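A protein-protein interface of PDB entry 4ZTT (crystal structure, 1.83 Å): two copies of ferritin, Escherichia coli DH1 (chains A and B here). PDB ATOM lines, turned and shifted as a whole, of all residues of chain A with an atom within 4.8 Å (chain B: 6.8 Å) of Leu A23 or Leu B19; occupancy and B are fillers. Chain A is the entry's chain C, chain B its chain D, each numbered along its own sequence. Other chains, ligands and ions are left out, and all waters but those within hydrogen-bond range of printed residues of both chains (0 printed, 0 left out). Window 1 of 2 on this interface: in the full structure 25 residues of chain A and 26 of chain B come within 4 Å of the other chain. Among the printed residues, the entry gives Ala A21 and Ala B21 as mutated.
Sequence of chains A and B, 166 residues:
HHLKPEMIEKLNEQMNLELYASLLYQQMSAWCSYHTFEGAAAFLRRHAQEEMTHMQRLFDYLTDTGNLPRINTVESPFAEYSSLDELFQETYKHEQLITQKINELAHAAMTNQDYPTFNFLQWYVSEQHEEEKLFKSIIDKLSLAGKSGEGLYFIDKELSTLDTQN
OE1 of Gln A27 lies within hydrogen-bond range of N of Ile B71 (2.8 Å).
N of Val A74 lies within hydrogen-bond range of O of Val B74.
Among the printed residues, merely in contact across the chains: Leu A19 with Leu B23 (3.95 Å), Leu A23 with Leu B19 (3.998 Å), Leu A23 with Ile B71 (3.8 Å), Gln A26 with Met B55 (3.9 Å), Gln A26 with Phe B59 (3.2 Å), Gln A26 with Ile B71 (3.97 Å) and Pro A77 with Ile B71 (3.4 Å).
Of the printed residues of chain B, Leu A23 touches Leu B19 (3.998 Å) and Ile B71 (3.8 Å).
Of the printed residues of chain A, Leu B19 touches Leu A23.
Of the printed residues of chain A, Leu B23 touches Leu A19 (3.95 Å).
Of the printed residues of chain B, Leu A19 touches Leu B23.
Of the printed residues of chain B, Gln A27 touches Ile B71.
Gln B14 touches none of the printed residues of chain A.
Met B52 touches none of the printed residues of chain A.
The nearest printed residue of chain A that does not touch Leu B19 is Leu A19 (5.9 Å).
The nearest printed residue of chain A that does not touch Phe B59 is Gln A27 (4.5 Å).
Hydrophobic or aromatic side chains of chain A within 4 Å of the printed part of chain B: Leu A19, Leu A23 and Pro A77.
Hydrophobic or aromatic side chains of chain B that line the printed part of chain A: Leu B19, Leu B23, Met B55, Phe B59 and Ile B71.
Among the printed residues, no Asp or Glu carboxylate lies within 4 Å of a Lys or Arg side-chain nitrogen of the other chain.
Leu A19 touches Leu B23, and with the chains exchanged Leu A23 touches Leu B19.
Val B74 touches its own counterpart, Val A74.
7 positions are printed for both chains.
Of the 9 pairs that touch across the chains among the printed residues, 3 have their exchanged pair printed and touching as well.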
ATOM      1  N   LEU A  19     -19.772  12.043  -3.018  1.00  0.00           N
ATOM      2  CA  LEU A  19     -20.802  11.983  -1.956  1.00  0.00           C
ATOM      3  C   LEU A  19     -20.348  11.092  -0.775  1.00  0.00           C
ATOM      4  O   LEU A  19     -20.458  11.523   0.393  1.00  0.00           O
ATOM      5  CB  LEU A  19     -22.111  11.400  -2.551  1.00  0.00           C
ATOM      6  CG  LEU A  19     -23.201  11.132  -1.457  1.00  0.00           C
ATOM      7  CD1 LEU A  19     -23.534  12.401  -0.652  1.00  0.00           C
ATOM      8  CD2 LEU A  19     -24.430  10.611  -2.129  1.00  0.00           C
ATOM      9  N   TYR A  20     -19.860   9.881  -1.074  1.00  0.00           N
ATOM     10  CA  TYR A  20     -19.292   9.022  -0.094  1.00  0.00           C
ATOM     11  C   TYR A  20     -18.202   9.749   0.713  1.00  0.00           C
ATOM     12  O   TYR A  20     -18.188   9.592   1.943  1.00  0.00           O
ATOM     13  CB  TYR A  20     -18.838   7.691  -0.591  1.00  0.00           C
ATOM     14  CG  TYR A  20     -18.307   6.829   0.482  1.00  0.00           C
ATOM     15  CD1 TYR A  20     -19.167   6.062   1.273  1.00  0.00           C
ATOM     16  CD2 TYR A  20     -16.958   6.745   0.729  1.00  0.00           C
ATOM     17  CE1 TYR A  20     -18.629   5.245   2.263  1.00  0.00           C
ATOM     18  CE2 TYR A  20     -16.473   5.973   1.749  1.00  0.00           C
ATOM     19  CZ  TYR A  20     -17.318   5.231   2.501  1.00  0.00           C
ATOM     20  OH  TYR A  20     -16.824   4.448   3.579  1.00  0.00           O
ATOM     21  N   ALA A  21     -17.251  10.381   0.013  1.00  0.00           N
ATOM     22  CA  ALA A  21     -16.185  11.113   0.674  1.00  0.00           C
ATOM     23  C   ALA A  21     -16.783  12.135   1.671  1.00  0.00           C
ATOM     24  O   ALA A  21     -16.247  12.334   2.780  1.00  0.00           O
ATOM     25  CB  ALA A  21     -15.368  11.848  -0.329  1.00  0.00           C
ATOM     26  N   SER A  22     -17.815  12.867   1.226  1.00  0.00           N
ATOM     27  CA  SER A  22     -18.519  13.797   2.126  1.00  0.00           C
ATOM     28  C   SER A  22     -18.941  13.086   3.405  1.00  0.00           C
ATOM     29  O   SER A  22     -18.693  13.591   4.513  1.00  0.00           O
ATOM     30  CB  SER A  22     -19.645  14.538   1.416  1.00  0.00           C
ATOM     31  OG  SER A  22     -20.228  15.473   2.279  1.00  0.00           O
ATOM     32  N   LEU A  23     -19.724  12.018   3.290  1.00  0.00           N
ATOM     33  CA  LEU A  23     -20.284  11.404   4.423  1.00  0.00           C
ATOM     34  C   LEU A  23     -19.200  10.689   5.266  1.00  0.00           C
ATOM     35  O   LEU A  23     -19.301  10.633   6.515  1.00  0.00           O
ATOM     36  CB  LEU A  23     -21.332  10.390   4.012  1.00  0.00           C
ATOM     37  CG  LEU A  23     -22.436  11.004   3.188  1.00  0.00           C
ATOM     38  CD1 LEU A  23     -23.430   9.935   2.734  1.00  0.00           C
ATOM     39  CD2 LEU A  23     -23.111  12.147   3.922  1.00  0.00           C
ATOM     40  N   LEU A  24     -18.145  10.251   4.609  1.00  0.00           N
ATOM     41  CA  LEU A  24     -17.008   9.732   5.316  1.00  0.00           C
ATOM     42  C   LEU A  24     -16.369  10.740   6.237  1.00  0.00           C
ATOM     43  O   LEU A  24     -16.122  10.390   7.402  1.00  0.00           O
ATOM     44  CB  LEU A  24     -15.946   9.108   4.419  1.00  0.00           C
ATOM     45  CG  LEU A  24     -14.660   8.555   5.074  1.00  0.00           C
ATOM     46  CD1 LEU A  24     -15.055   7.347   5.865  1.00  0.00           C
ATOM     47  CD2 LEU A  24     -13.619   8.194   3.982  1.00  0.00           C
ATOM     48  N   TYR A  25     -16.087  11.922   5.748  1.00  0.00           N
ATOM     49  CA  TYR A  25     -15.402  12.965   6.499  1.00  0.00           C
ATOM     50  C   TYR A  25     -16.341  13.485   7.593  1.00  0.00           C
ATOM     51  O   TYR A  25     -15.876  13.781   8.689  1.00  0.00           O
ATOM     52  CB  TYR A  25     -14.896  14.074   5.574  1.00  0.00           C
ATOM     53  CG  TYR A  25     -13.902  13.600   4.531  1.00  0.00           C
ATOM     54  CD1 TYR A  25     -13.198  12.397   4.652  1.00  0.00           C
ATOM     55  CD2 TYR A  25     -13.663  14.336   3.392  1.00  0.00           C
ATOM     56  CE1 TYR A  25     -12.368  11.959   3.645  1.00  0.00           C
ATOM     57  CE2 TYR A  25     -12.805  13.905   2.422  1.00  0.00           C
ATOM     58  CZ  TYR A  25     -12.136  12.721   2.549  1.00  0.00           C
ATOM     59  OH  TYR A  25     -11.299  12.296   1.483  1.00  0.00           O
ATOM     60  N   GLN A  26     -17.640  13.505   7.296  1.00  0.00           N
ATOM     61  CA  GLN A  26     -18.662  13.890   8.265  1.00  0.00           C
ATOM     62  C   GLN A  26     -18.594  12.868   9.407  1.00  0.00           C
ATOM     63  O   GLN A  26     -18.490  13.251  10.555  1.00  0.00           O
ATOM     64  CB  GLN A  26     -20.025  13.975   7.675  1.00  0.00           C
ATOM     65  CG  GLN A  26     -21.048  14.463   8.675  1.00  0.00           C
ATOM     66  CD  GLN A  26     -20.947  15.930   8.995  1.00  0.00           C
ATOM     67  OE1 GLN A  26     -20.577  16.707   8.159  1.00  0.00           O
ATOM     68  NE2 GLN A  26     -21.310  16.301  10.177  1.00  0.00           N
ATOM     69  N   GLN A  27     -18.614  11.595   9.095  1.00  0.00           N
ATOM     70  CA  GLN A  27     -18.545  10.548  10.108  1.00  0.00           C
ATOM     71  C   GLN A  27     -17.273  10.562  10.904  1.00  0.00           C
ATOM     72  O   GLN A  27     -17.297  10.497  12.135  1.00  0.00           O
ATOM     73  CB  GLN A  27     -18.746   9.214   9.504  1.00  0.00           C
ATOM     74  CG  GLN A  27     -18.839   8.056  10.528  1.00  0.00           C
ATOM     75  CD  GLN A  27     -20.119   8.199  11.366  1.00  0.00           C
ATOM     76  OE1 GLN A  27     -21.205   8.177  10.837  1.00  0.00           O
ATOM     77  NE2 GLN A  27     -19.996   8.296  12.659  1.00  0.00           N
ATOM     78  N   VAL A  74     -25.827   4.345  -0.451  1.00  0.00           N
ATOM     79  CA  VAL A  74     -24.494   4.730   0.070  1.00  0.00           C
ATOM     80  C   VAL A  74     -24.258   3.819   1.258  1.00  0.00           C
ATOM     81  O   VAL A  74     -25.013   3.798   2.226  1.00  0.00           O
ATOM     82  CB  VAL A  74     -24.457   6.186   0.529  1.00  0.00           C
ATOM     83  CG1 VAL A  74     -23.051   6.545   1.059  1.00  0.00           C
ATOM     84  CG2 VAL A  74     -24.860   7.155  -0.612  1.00  0.00           C
ATOM     85  N   PRO A  77     -20.597   4.901   6.313  1.00  0.00           N
ATOM     86  CA  PRO A  77     -19.133   5.152   6.426  1.00  0.00           C
ATOM     87  C   PRO A  77     -18.529   4.836   7.781  1.00  0.00           C
ATOM     88  O   PRO A  77     -17.402   5.223   8.035  1.00  0.00           O
ATOM     89  CB  PRO A  77     -19.011   6.648   6.162  1.00  0.00           C
ATOM     90  CG  PRO A  77     -20.332   7.207   6.627  1.00  0.00           C
ATOM     91  CD  PRO A  77     -21.368   6.155   6.284  1.00  0.00           C
ATOM     92  N   GLN B  14     -33.444  10.359  13.293  1.00  0.00           N
ATOM     93  CA  GLN B  14     -33.830  11.626  12.659  1.00  0.00           C
ATOM     94  C   GLN B  14     -32.737  12.300  11.906  1.00  0.00           C
ATOM     95  O   GLN B  14     -32.959  12.862  10.831  1.00  0.00           O
ATOM     96  CB  GLN B  14     -34.414  12.560  13.696  1.00  0.00           C
ATOM     97  CG  GLN B  14     -35.025  13.873  13.175  1.00  0.00           C
ATOM     98  CD  GLN B  14     -36.287  13.659  12.338  1.00  0.00           C
ATOM     99  OE1 GLN B  14     -37.037  12.761  12.573  1.00  0.00           O
ATOM    100  NE2 GLN B  14     -36.522  14.550  11.386  1.00  0.00           N
ATOM    101  N   MET B  15     -31.550  12.312  12.453  1.00  0.00           N
ATOM    102  CA  MET B  15     -30.384  12.748  11.700  1.00  0.00           C
ATOM    103  C   MET B  15     -30.318  12.087  10.304  1.00  0.00           C
ATOM    104  O   MET B  15     -30.115  12.767   9.316  1.00  0.00           O
ATOM    105  CB  MET B  15     -29.144  12.435  12.483  1.00  0.00           C
ATOM    106  CG  MET B  15     -27.881  13.159  11.953  1.00  0.00           C
ATOM    107  SD  MET B  15     -26.422  12.481  12.713  1.00  0.00           S
ATOM    108  CE  MET B  15     -26.479  10.746  12.256  1.00  0.00           C
ATOM    109  N   ASN B  16     -30.389  10.778  10.288  1.00  0.00           N
ATOM    110  CA  ASN B  16     -30.412   9.987   9.041  1.00  0.00           C
ATOM    111  C   ASN B  16     -31.588  10.298   8.132  1.00  0.00           C
ATOM    112  O   ASN B  16     -31.406  10.386   6.879  1.00  0.00           O
ATOM    113  CB  ASN B  16     -30.316   8.519   9.354  1.00  0.00           C
ATOM    114  CG  ASN B  16     -28.912   8.084   9.681  1.00  0.00           C
ATOM    115  OD1 ASN B  16     -28.175   7.732   8.778  1.00  0.00           O
ATOM    116  ND2 ASN B  16     -28.526   8.041  10.981  1.00  0.00           N
ATOM    117  N   LEU B  17     -32.765  10.620   8.724  1.00  0.00           N
ATOM    118  CA  LEU B  17     -33.939  10.981   7.913  1.00  0.00           C
ATOM    119  C   LEU B  17     -33.669  12.362   7.234  1.00  0.00           C
ATOM    120  O   LEU B  17     -34.042  12.550   6.069  1.00  0.00           O
ATOM    121  CB  LEU B  17     -35.248  10.958   8.728  1.00  0.00           C
ATOM    122  CG  LEU B  17     -36.508  11.424   8.037  1.00  0.00           C
ATOM    123  CD1 LEU B  17     -36.806  10.409   6.947  1.00  0.00           C
ATOM    124  CD2 LEU B  17     -37.645  11.600   9.023  1.00  0.00           C
ATOM    125  N   GLU B  18     -33.057  13.308   7.931  1.00  0.00           N
ATOM    126  CA  GLU B  18     -32.691  14.556   7.366  1.00  0.00           C
ATOM    127  C   GLU B  18     -31.668  14.421   6.198  1.00  0.00           C
ATOM    128  O   GLU B  18     -31.789  15.103   5.186  1.00  0.00           O
ATOM    129  CB  GLU B  18     -32.133  15.594   8.407  1.00  0.00           C
ATOM    130  CG  GLU B  18     -33.031  15.969   9.608  1.00  0.00           C
ATOM    131  CD  GLU B  18     -34.339  16.697   9.262  1.00  0.00           C
ATOM    132  OE1 GLU B  18     -34.353  17.383   8.183  1.00  0.00           O
ATOM    133  OE2 GLU B  18     -35.317  16.672  10.053  1.00  0.00           O
ATOM    134  N   LEU B  19     -30.653  13.591   6.391  1.00  0.00           N
ATOM    135  CA  LEU B  19     -29.741  13.206   5.340  1.00  0.00           C
ATOM    136  C   LEU B  19     -30.469  12.597   4.124  1.00  0.00           C
ATOM    137  O   LEU B  19     -30.161  13.039   2.993  1.00  0.00           O
ATOM    138  CB  LEU B  19     -28.650  12.270   5.922  1.00  0.00           C
ATOM    139  CG  LEU B  19     -27.702  11.693   4.844  1.00  0.00           C
ATOM    140  CD1 LEU B  19     -27.045  12.836   4.108  1.00  0.00           C
ATOM    141  CD2 LEU B  19     -26.648  10.920   5.656  1.00  0.00           C
ATOM    142  N   TYR B  20     -31.395  11.705   4.350  1.00  0.00           N
ATOM    143  CA  TYR B  20     -32.156  11.105   3.313  1.00  0.00           C
ATOM    144  C   TYR B  20     -32.942  12.209   2.576  1.00  0.00           C
ATOM    145  O   TYR B  20     -32.983  12.178   1.401  1.00  0.00           O
ATOM    146  CB  TYR B  20     -33.094  10.056   3.787  1.00  0.00           C
ATOM    147  CG  TYR B  20     -33.861   9.454   2.628  1.00  0.00           C
ATOM    148  CD1 TYR B  20     -33.268   8.529   1.788  1.00  0.00           C
ATOM    149  CD2 TYR B  20     -35.157   9.839   2.339  1.00  0.00           C
ATOM    150  CE1 TYR B  20     -33.940   7.969   0.739  1.00  0.00           C
ATOM    151  CE2 TYR B  20     -35.852   9.278   1.263  1.00  0.00           C
ATOM    152  CZ  TYR B  20     -35.240   8.373   0.461  1.00  0.00           C
ATOM    153  OH  TYR B  20     -35.909   7.876  -0.631  1.00  0.00           O
ATOM    154  N   ALA B  21     -33.588  13.105   3.283  1.00  0.00           N
ATOM    155  CA  ALA B  21     -34.312  14.210   2.661  1.00  0.00           C
ATOM    156  C   ALA B  21     -33.411  14.986   1.737  1.00  0.00           C
ATOM    157  O   ALA B  21     -33.879  15.406   0.690  1.00  0.00           O
ATOM    158  CB  ALA B  21     -34.857  15.169   3.705  1.00  0.00           C
ATOM    159  N   SER B  22     -32.213  15.391   2.232  1.00  0.00           N
ATOM    160  CA  SER B  22     -31.192  15.977   1.380  1.00  0.00           C
ATOM    161  C   SER B  22     -30.955  15.284   0.056  1.00  0.00           C
ATOM    162  O   SER B  22     -31.104  15.935  -0.999  1.00  0.00           O
ATOM    163  CB  SER B  22     -29.879  16.256   2.120  1.00  0.00           C
ATOM    164  OG  SER B  22     -29.035  17.053   1.299  1.00  0.00           O
ATOM    165  N   LEU B  23     -30.708  13.988   0.121  1.00  0.00           N
ATOM    166  CA  LEU B  23     -30.397  13.142  -1.046  1.00  0.00           C
ATOM    167  C   LEU B  23     -31.629  12.965  -1.917  1.00  0.00           C
ATOM    168  O   LEU B  23     -31.529  13.068  -3.133  1.00  0.00           O
ATOM    169  CB  LEU B  23     -29.761  11.830  -0.622  1.00  0.00           C
ATOM    170  CG  LEU B  23     -28.430  12.105   0.140  1.00  0.00           C
ATOM    171  CD1 LEU B  23     -27.942  10.746   0.531  1.00  0.00           C
ATOM    172  CD2 LEU B  23     -27.457  12.892  -0.695  1.00  0.00           C
ATOM    173  N   LEU B  24     -32.785  12.827  -1.319  1.00  0.00           N
ATOM    174  CA  LEU B  24     -34.001  12.826  -2.069  1.00  0.00           C
ATOM    175  C   LEU B  24     -34.280  14.096  -2.900  1.00  0.00           C
ATOM    176  O   LEU B  24     -34.490  13.940  -4.085  1.00  0.00           O
ATOM    177  CB  LEU B  24     -35.201  12.486  -1.174  1.00  0.00           C
ATOM    178  CG  LEU B  24     -36.648  12.518  -1.731  1.00  0.00           C
ATOM    179  CD1 LEU B  24     -36.784  11.420  -2.754  1.00  0.00           C
ATOM    180  CD2 LEU B  24     -37.725  12.315  -0.605  1.00  0.00           C
ATOM    181  N   ALA B  48     -31.988  20.902  -0.860  1.00  0.00           N
ATOM    182  CA  ALA B  48     -31.164  19.829  -0.464  1.00  0.00           C
ATOM    183  C   ALA B  48     -30.060  20.297   0.490  1.00  0.00           C
ATOM    184  O   ALA B  48     -29.678  19.574   1.432  1.00  0.00           O
ATOM    185  CB  ALA B  48     -30.629  19.101  -1.658  1.00  0.00           C
ATOM    186  N   GLU B  51     -31.488  20.902   3.916  1.00  0.00           N
ATOM    187  CA  GLU B  51     -31.632  19.618   4.666  1.00  0.00           C
ATOM    188  C   GLU B  51     -30.377  19.143   5.266  1.00  0.00           C
ATOM    189  O   GLU B  51     -30.367  18.571   6.400  1.00  0.00           O
ATOM    190  CB  GLU B  51     -32.275  18.529   3.769  1.00  0.00           C
ATOM    191  CG  GLU B  51     -33.687  18.821   3.314  1.00  0.00           C
ATOM    192  CD  GLU B  51     -34.697  19.026   4.439  1.00  0.00           C
ATOM    193  OE1 GLU B  51     -34.529  18.580   5.614  1.00  0.00           O
ATOM    194  OE2 GLU B  51     -35.708  19.634   4.096  1.00  0.00           O
ATOM    195  N   MET B  52     -29.247  19.332   4.573  1.00  0.00           N
ATOM    196  CA  MET B  52     -27.961  18.984   5.169  1.00  0.00           C
ATOM    197  C   MET B  52     -27.709  19.779   6.431  1.00  0.00           C
ATOM    198  O   MET B  52     -27.086  19.274   7.349  1.00  0.00           O
ATOM    199  CB  MET B  52     -26.803  19.246   4.195  1.00  0.00           C
ATOM    200  CG  MET B  52     -26.656  18.184   3.144  1.00  0.00           C
ATOM    201  SD  MET B  52     -26.433  16.551   3.847  1.00  0.00           S
ATOM    202  CE  MET B  52     -24.994  16.901   4.708  1.00  0.00           C
ATOM    203  N   HIS B  54     -30.001  20.756   8.494  1.00  0.00           N
ATOM    204  CA  HIS B  54     -30.807  20.126   9.500  1.00  0.00           C
ATOM    205  C   HIS B  54     -30.144  18.845  10.052  1.00  0.00           C
ATOM    206  O   HIS B  54     -30.266  18.566  11.255  1.00  0.00           O
ATOM    207  CB  HIS B  54     -32.192  19.709   8.993  1.00  0.00           C
ATOM    208  CG  HIS B  54     -33.045  20.808   8.405  1.00  0.00           C
ATOM    209  ND1 HIS B  54     -34.270  20.534   7.749  1.00  0.00           N
ATOM    210  CD2 HIS B  54     -32.808  22.126   8.295  1.00  0.00           C
ATOM    211  CE1 HIS B  54     -34.705  21.694   7.294  1.00  0.00           C
ATOM    212  NE2 HIS B  54     -33.855  22.657   7.635  1.00  0.00           N
ATOM    213  N   MET B  55     -29.450  18.091   9.201  1.00  0.00           N
ATOM    214  CA  MET B  55     -28.607  16.969   9.690  1.00  0.00           C
ATOM    215  C   MET B  55     -27.516  17.501  10.632  1.00  0.00           C
ATOM    216  O   MET B  55     -27.401  17.074  11.761  1.00  0.00           O
ATOM    217  CB  MET B  55     -28.018  16.228   8.507  1.00  0.00           C
ATOM    218  CG  MET B  55     -27.301  14.900   8.822  1.00  0.00           C
ATOM    219  SD  MET B  55     -25.875  14.732   7.735  1.00  0.00           S
ATOM    220  CE  MET B  55     -24.853  15.921   8.615  1.00  0.00           C
ATOM    221  N   PHE B  59     -26.614  16.102  14.335  1.00  0.00           N
ATOM    222  CA  PHE B  59     -25.253  15.504  14.438  1.00  0.00           C
ATOM    223  C   PHE B  59     -24.542  16.189  15.627  1.00  0.00           C
ATOM    224  O   PHE B  59     -23.970  15.526  16.485  1.00  0.00           O
ATOM    225  CB  PHE B  59     -24.539  15.724  13.102  1.00  0.00           C
ATOM    226  CG  PHE B  59     -23.341  14.858  12.908  1.00  0.00           C
ATOM    227  CD1 PHE B  59     -22.190  15.261  13.471  1.00  0.00           C
ATOM    228  CD2 PHE B  59     -23.379  13.688  12.185  1.00  0.00           C
ATOM    229  CE1 PHE B  59     -20.978  14.546  13.231  1.00  0.00           C
ATOM    230  CE2 PHE B  59     -22.214  12.952  11.996  1.00  0.00           C
ATOM    231  CZ  PHE B  59     -21.037  13.405  12.551  1.00  0.00           C
ATOM    232  N   ILE B  71     -23.956   7.686  10.749  1.00  0.00           N
ATOM    233  CA  ILE B  71     -24.577   7.735   9.401  1.00  0.00           C
ATOM    234  C   ILE B  71     -24.718   6.287   8.967  1.00  0.00           C
ATOM    235  O   ILE B  71     -23.685   5.536   8.756  1.00  0.00           O
ATOM    236  CB  ILE B  71     -23.724   8.544   8.412  1.00  0.00           C
ATOM    237  CG1 ILE B  71     -23.728   9.998   8.801  1.00  0.00           C
ATOM    238  CG2 ILE B  71     -24.335   8.446   7.010  1.00  0.00           C
ATOM    239  CD1 ILE B  71     -22.713  10.901   8.120  1.00  0.00           C
ATOM    240  N   ASN B  72     -25.970   5.871   8.886  1.00  0.00           N
ATOM    241  CA  ASN B  72     -26.290   4.525   8.516  1.00  0.00           C
ATOM    242  C   ASN B  72     -26.332   4.424   6.990  1.00  0.00           C
ATOM    243  O   ASN B  72     -26.273   5.482   6.332  1.00  0.00           O
ATOM    244  CB  ASN B  72     -27.640   4.155   9.075  1.00  0.00           C
ATOM    245  CG  ASN B  72     -27.647   4.066  10.623  1.00  0.00           C
ATOM    246  OD1 ASN B  72     -26.689   3.653  11.259  1.00  0.00           O
ATOM    247  ND2 ASN B  72     -28.739   4.529  11.190  1.00  0.00           N
ATOM    248  N   VAL B  74     -27.658   4.538   3.465  1.00  0.00           N
ATOM    249  CA  VAL B  74     -28.775   5.332   2.865  1.00  0.00           C
ATOM    250  C   VAL B  74     -29.230   4.620   1.589  1.00  0.00           C
ATOM    251  O   VAL B  74     -28.486   4.449   0.666  1.00  0.00           O
ATOM    252  CB  VAL B  74     -28.337   6.747   2.469  1.00  0.00           C
ATOM    253  CG1 VAL B  74     -29.607   7.566   2.134  1.00  0.00           C
ATOM    254  CG2 VAL B  74     -27.508   7.367   3.571  1.00  0.00           C
